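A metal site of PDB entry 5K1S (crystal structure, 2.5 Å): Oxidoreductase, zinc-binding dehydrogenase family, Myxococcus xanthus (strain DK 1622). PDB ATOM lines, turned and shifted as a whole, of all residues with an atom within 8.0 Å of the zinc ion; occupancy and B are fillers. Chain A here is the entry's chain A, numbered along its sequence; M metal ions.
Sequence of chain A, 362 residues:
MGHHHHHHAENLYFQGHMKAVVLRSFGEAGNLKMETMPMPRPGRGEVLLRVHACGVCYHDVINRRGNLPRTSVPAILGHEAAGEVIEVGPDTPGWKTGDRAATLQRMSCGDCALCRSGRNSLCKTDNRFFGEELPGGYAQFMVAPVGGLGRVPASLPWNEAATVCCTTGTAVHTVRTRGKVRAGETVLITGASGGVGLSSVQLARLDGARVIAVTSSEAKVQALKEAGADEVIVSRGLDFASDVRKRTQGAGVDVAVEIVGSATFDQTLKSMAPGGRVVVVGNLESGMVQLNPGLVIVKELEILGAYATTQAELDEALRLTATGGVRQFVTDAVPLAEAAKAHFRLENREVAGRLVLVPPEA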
ATOM      1  N   ARG A 106      21.884  -1.137   7.687  1.00  0.00           N
ATOM      2  CA  ARG A 106      22.425  -2.432   7.329  1.00  0.00           C
ATOM      3  C   ARG A 106      21.954  -2.812   5.933  1.00  0.00           C
ATOM      4  O   ARG A 106      21.009  -2.237   5.389  1.00  0.00           O
ATOM      5  CB  ARG A 106      22.013  -3.516   8.339  1.00  0.00           C
ATOM      6  CG  ARG A 106      20.505  -3.694   8.447  1.00  0.00           C
ATOM      7  CD  ARG A 106      20.129  -4.804   9.416  1.00  0.00           C
ATOM      8  NE  ARG A 106      20.489  -6.127   8.907  1.00  0.00           N
ATOM      9  CZ  ARG A 106      19.808  -6.789   7.979  1.00  0.00           C
ATOM     10  NH1 ARG A 106      18.724  -6.252   7.441  1.00  0.00           N
ATOM     11  NH2 ARG A 106      20.209  -7.989   7.591  1.00  0.00           N
ATOM     12  N   MET A 107      22.612  -3.829   5.370  1.00  0.00           N
ATOM     13  CA  MET A 107      22.283  -4.309   4.045  1.00  0.00           C
ATOM     14  C   MET A 107      21.219  -5.405   4.126  1.00  0.00           C
ATOM     15  O   MET A 107      20.749  -5.782   5.196  1.00  0.00           O
ATOM     16  CB  MET A 107      23.542  -4.835   3.342  1.00  0.00           C
ATOM     17  CG  MET A 107      24.466  -3.748   2.818  1.00  0.00           C
ATOM     18  SD  MET A 107      23.637  -2.621   1.692  1.00  0.00           S
ATOM     19  CE  MET A 107      23.099  -3.743   0.403  1.00  0.00           C
ATOM     20  N   SER A 108      20.852  -5.925   2.957  1.00  0.00           N
ATOM     21  CA  SER A 108      19.835  -6.972   2.843  1.00  0.00           C
ATOM     22  C   SER A 108      20.010  -7.627   1.480  1.00  0.00           C
ATOM     23  O   SER A 108      20.100  -6.934   0.470  1.00  0.00           O
ATOM     24  CB  SER A 108      18.427  -6.388   3.000  1.00  0.00           C
ATOM     25  OG  SER A 108      17.437  -7.388   2.851  1.00  0.00           O
ATOM     26  N   CYS A 109      20.063  -8.965   1.463  1.00  0.00           N
ATOM     27  CA  CYS A 109      20.393  -9.664   0.225  1.00  0.00           C
ATOM     28  C   CYS A 109      19.333  -9.426  -0.841  1.00  0.00           C
ATOM     29  O   CYS A 109      19.648  -9.138  -2.000  1.00  0.00           O
ATOM     30  CB  CYS A 109      20.568 -11.150   0.495  1.00  0.00           C
ATOM     31  SG  CYS A 109      19.033 -12.075   0.762  1.00  0.00           S
ATOM     32  N   GLY A 110      18.063  -9.540  -0.472  1.00  0.00           N
ATOM     33  CA  GLY A 110      16.966  -9.313  -1.393  1.00  0.00           C
ATOM     34  C   GLY A 110      16.415 -10.559  -2.056  1.00  0.00           C
ATOM     35  O   GLY A 110      15.465 -10.446  -2.847  1.00  0.00           O
ATOM     36  N   ASP A 111      16.967 -11.735  -1.772  1.00  0.00           N
ATOM     37  CA  ASP A 111      16.587 -12.972  -2.440  1.00  0.00           C
ATOM     38  C   ASP A 111      15.978 -14.014  -1.523  1.00  0.00           C
ATOM     39  O   ASP A 111      15.188 -14.832  -1.987  1.00  0.00           O
ATOM     40  CB  ASP A 111      17.806 -13.584  -3.144  1.00  0.00           C
ATOM     41  CG  ASP A 111      18.369 -12.683  -4.221  1.00  0.00           C
ATOM     42  OD1 ASP A 111      17.577 -11.975  -4.885  1.00  0.00           O
ATOM     43  OD2 ASP A 111      19.611 -12.672  -4.405  1.00  0.00           O
ATOM     44  N   CYS A 112      16.334 -14.019  -0.240  1.00  0.00           N
ATOM     45  CA  CYS A 112      15.783 -15.008   0.676  1.00  0.00           C
ATOM     46  C   CYS A 112      14.297 -14.747   0.916  1.00  0.00           C
ATOM     47  O   CYS A 112      13.768 -13.683   0.612  1.00  0.00           O
ATOM     48  CB  CYS A 112      16.545 -14.990   2.005  1.00  0.00           C
ATOM     49  SG  CYS A 112      16.270 -13.504   3.003  1.00  0.00           S
ATOM     50  N   ALA A 113      13.631 -15.764   1.468  1.00  0.00           N
ATOM     51  CA  ALA A 113      12.190 -15.653   1.727  1.00  0.00           C
ATOM     52  C   ALA A 113      11.863 -14.371   2.488  1.00  0.00           C
ATOM     53  O   ALA A 113      10.940 -13.638   2.121  1.00  0.00           O
ATOM     54  CB  ALA A 113      11.720 -16.880   2.502  1.00  0.00           C
ATOM     55  N   LEU A 114      12.613 -14.092   3.551  1.00  0.00           N
ATOM     56  CA  LEU A 114      12.334 -12.921   4.379  1.00  0.00           C
ATOM     57  C   LEU A 114      12.384 -11.648   3.552  1.00  0.00           C
ATOM     58  O   LEU A 114      11.485 -10.803   3.642  1.00  0.00           O
ATOM     59  CB  LEU A 114      13.313 -12.858   5.545  1.00  0.00           C
ATOM     60  CG  LEU A 114      13.201 -13.989   6.553  1.00  0.00           C
ATOM     61  CD1 LEU A 114      14.463 -14.092   7.394  1.00  0.00           C
ATOM     62  CD2 LEU A 114      11.986 -13.773   7.451  1.00  0.00           C
ATOM     63  N   CYS A 115      13.433 -11.482   2.751  1.00  0.00           N
ATOM     64  CA  CYS A 115      13.534 -10.305   1.888  1.00  0.00           C
ATOM     65  C   CYS A 115      12.367 -10.238   0.918  1.00  0.00           C
ATOM     66  O   CYS A 115      11.743  -9.183   0.737  1.00  0.00           O
ATOM     67  CB  CYS A 115      14.861 -10.322   1.130  1.00  0.00           C
ATOM     68  SG  CYS A 115      16.308  -9.826   2.111  1.00  0.00           S
ATOM     69  N   ARG A 116      12.048 -11.371   0.268  1.00  0.00           N
ATOM     70  CA  ARG A 116      10.936 -11.391  -0.671  1.00  0.00           C
ATOM     71  C   ARG A 116       9.612 -11.069  -0.001  1.00  0.00           C
ATOM     72  O   ARG A 116       8.644 -10.712  -0.691  1.00  0.00           O
ATOM     73  CB  ARG A 116      10.847 -12.758  -1.362  1.00  0.00           C
ATOM     74  CG  ARG A 116      12.115 -13.176  -2.111  1.00  0.00           C
ATOM     75  CD  ARG A 116      11.845 -14.301  -3.099  1.00  0.00           C
ATOM     76  NE  ARG A 116      11.207 -15.453  -2.479  1.00  0.00           N
ATOM     77  CZ  ARG A 116      11.852 -16.475  -1.913  1.00  0.00           C
ATOM     78  NH1 ARG A 116      11.168 -17.477  -1.377  1.00  0.00           N
ATOM     79  NH2 ARG A 116      13.184 -16.490  -1.870  1.00  0.00           N
ATOM     80  N   ARG A 119      10.461  -8.346   4.758  1.00  0.00           N
ATOM     81  CA  ARG A 119      11.071  -8.394   6.092  1.00  0.00           C
ATOM     82  C   ARG A 119      12.588  -8.253   6.003  1.00  0.00           C
ATOM     83  O   ARG A 119      13.328  -9.026   6.599  1.00  0.00           O
ATOM     84  CB  ARG A 119      10.683  -9.686   6.802  1.00  0.00           C
ATOM     85  CG  ARG A 119       9.207 -10.043   6.715  1.00  0.00           C
ATOM     86  CD  ARG A 119       8.329  -8.982   7.367  1.00  0.00           C
ATOM     87  NE  ARG A 119       8.627  -8.815   8.777  1.00  0.00           N
ATOM     88  CZ  ARG A 119       8.118  -9.562   9.752  1.00  0.00           C
ATOM     89  NH1 ARG A 119       8.450  -9.323  11.019  1.00  0.00           N
ATOM     90  NH2 ARG A 119       7.295 -10.565   9.475  1.00  0.00           N
ATOM     91  N   ASN A 120      13.046  -7.254   5.249  1.00  0.00           N
ATOM     92  CA  ASN A 120      14.488  -7.088   5.040  1.00  0.00           C
ATOM     93  C   ASN A 120      15.231  -6.915   6.362  1.00  0.00           C
ATOM     94  O   ASN A 120      16.396  -7.320   6.471  1.00  0.00           O
ATOM     95  CB  ASN A 120      14.746  -5.889   4.124  1.00  0.00           C
ATOM     96  CG  ASN A 120      14.048  -6.030   2.783  1.00  0.00           C
ATOM     97  OD1 ASN A 120      13.019  -6.692   2.673  1.00  0.00           O
ATOM     98  ND2 ASN A 120      14.609  -5.395   1.756  1.00  0.00           N
ATOM     99  N   SER A 121      14.588  -6.311   7.369  1.00  0.00           N
ATOM    100  CA  SER A 121      15.229  -6.161   8.671  1.00  0.00           C
ATOM    101  C   SER A 121      15.679  -7.491   9.248  1.00  0.00           C
ATOM    102  O   SER A 121      16.597  -7.513  10.062  1.00  0.00           O
ATOM    103  CB  SER A 121      14.264  -5.473   9.641  1.00  0.00           C
ATOM    104  OG  SER A 121      13.919  -4.175   9.192  1.00  0.00           O
ATOM    105  N   LEU A 122      15.052  -8.599   8.828  1.00  0.00           N
ATOM    106  CA  LEU A 122      15.329  -9.915   9.387  1.00  0.00           C
ATOM    107  C   LEU A 122      16.236 -10.762   8.506  1.00  0.00           C
ATOM    108  O   LEU A 122      16.492 -11.924   8.845  1.00  0.00           O
ATOM    109  CB  LEU A 122      14.017 -10.659   9.628  1.00  0.00           C
ATOM    110  CG  LEU A 122      12.981  -9.910  10.470  1.00  0.00           C
ATOM    111  CD1 LEU A 122      11.686 -10.712  10.561  1.00  0.00           C
ATOM    112  CD2 LEU A 122      13.516  -9.607  11.859  1.00  0.00           C
ATOM    113  N   CYS A 123      16.731 -10.219   7.402  1.00  0.00           N
ATOM    114  CA  CYS A 123      17.593 -10.989   6.506  1.00  0.00           C
ATOM    115  C   CYS A 123      18.834 -11.468   7.239  1.00  0.00           C
ATOM    116  O   CYS A 123      19.496 -10.694   7.930  1.00  0.00           O
ATOM    117  CB  CYS A 123      17.988 -10.143   5.300  1.00  0.00           C
ATOM    118  SG  CYS A 123      19.163 -10.954   4.180  1.00  0.00           S
ATOM    119  N   LYS A 124      19.152 -12.760   7.082  1.00  0.00           N
ATOM    120  CA  LYS A 124      20.338 -13.341   7.691  1.00  0.00           C
ATOM    121  C   LYS A 124      21.482 -13.534   6.704  1.00  0.00           C
ATOM    122  O   LYS A 124      22.635 -13.689   7.141  1.00  0.00           O
ATOM    123  CB  LYS A 124      20.014 -14.689   8.337  1.00  0.00           C
ATOM    124  CG  LYS A 124      19.193 -14.597   9.621  1.00  0.00           C
ATOM    125  CD  LYS A 124      18.972 -15.971  10.227  1.00  0.00           C
ATOM    126  CE  LYS A 124      18.333 -15.880  11.609  1.00  0.00           C
ATOM    127  NZ  LYS A 124      18.055 -17.227  12.192  1.00  0.00           N
ATOM    128  N   THR A 125      21.212 -13.530   5.400  1.00  0.00           N
ATOM    129  CA  THR A 125      22.258 -13.818   4.420  1.00  0.00           C
ATOM    130  C   THR A 125      23.155 -12.616   4.164  1.00  0.00           C
ATOM    131  O   THR A 125      24.321 -12.802   3.788  1.00  0.00           O
ATOM    132  CB  THR A 125      21.625 -14.288   3.106  1.00  0.00           C
ATOM    133  OG1 THR A 125      20.819 -13.234   2.550  1.00  0.00           O
ATOM    134  CG2 THR A 125      20.748 -15.512   3.334  1.00  0.00           C
ATOM    135  N   ASP A 126      22.648 -11.405   4.352  1.00  0.00           N
ATOM    136  CA  ASP A 126      23.462 -10.184   4.219  1.00  0.00           C
ATOM    137  C   ASP A 126      23.069  -9.247   5.353  1.00  0.00           C
ATOM    138  O   ASP A 126      22.053  -8.545   5.261  1.00  0.00           O
ATOM    139  CB  ASP A 126      23.271  -9.524   2.862  1.00  0.00           C
ATOM    140  CG  ASP A 126      24.212  -8.360   2.645  1.00  0.00           C
ATOM    141  OD1 ASP A 126      24.850  -7.907   3.622  1.00  0.00           O
ATOM    142  OD2 ASP A 126      24.310  -7.868   1.496  1.00  0.00           O
ATOM    143  N   ASN A 127      23.862  -9.241   6.421  1.00  0.00           N
ATOM    144  CA  ASN A 127      23.617  -8.379   7.583  1.00  0.00           C
ATOM    145  C   ASN A 127      24.727  -7.347   7.767  1.00  0.00           C
ATOM    146  O   ASN A 127      24.934  -6.869   8.887  1.00  0.00           O
ATOM    147  CB  ASN A 127      23.462  -9.228   8.844  1.00  0.00           C
ATOM    148  CG  ASN A 127      24.648 -10.144   9.083  1.00  0.00           C
ATOM    149  OD1 ASN A 127      25.682 -10.031   8.412  1.00  0.00           O
ATOM    150  ND2 ASN A 127      24.521 -11.048  10.046  1.00  0.00           N
HETATM  151 ZN    ZN M   1      17.540 -11.637   2.486  1.00  0.00          ZN
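Merely in contact with the zinc ion: Gly 110 (3.7 Å) and Thr 125 (3.6 Å). The nearest printed residue that does not touch the zinc ion is Ser 108 (4.3 Å).
N of Gly 110 lies close to SG of Cys 115, 3.1 Å away. SG of Cys 115 sits close to OG of Ser 108, at 2.8 Å. The backbone NH (N) of Leu 114 lies close to the side-chain sulfur (SG) of Cys 112, at 3.7 Å. The side-chain sulfur (SG) of Cys 109 lies close to the side-chain hydroxyl (OG1) of Thr 125 (2.8 Å). The side-chain sulfur (SG) of Cys 109 lies close to the backbone NH (N) of Asp 111 (3.3 Å). The side-chain sulfur (SG) of Cys 123 sits close to the side-chain hydroxyl (OG1) of Thr 125 (3.3 Å). The side-chain sulfur (SG) of Cys 123 sits close to the backbone NH (N) of Asp 126 (3.5 Å). The guanidinium group of Arg 106 is in hydrogen-bond range of the backbone carbonyl oxygen of Cys 123 (2.8 Å).
The zinc ion is bound by the side-chain sulfur (SG) of Cys 115 (2.2 Å), the side-chain sulfur (SG) of Cys 112 (2.3 Å), the side-chain sulfur (SG) of Cys 109 (2.3 Å) and the side-chain sulfur (SG) of Cys 123 (2.4 Å).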
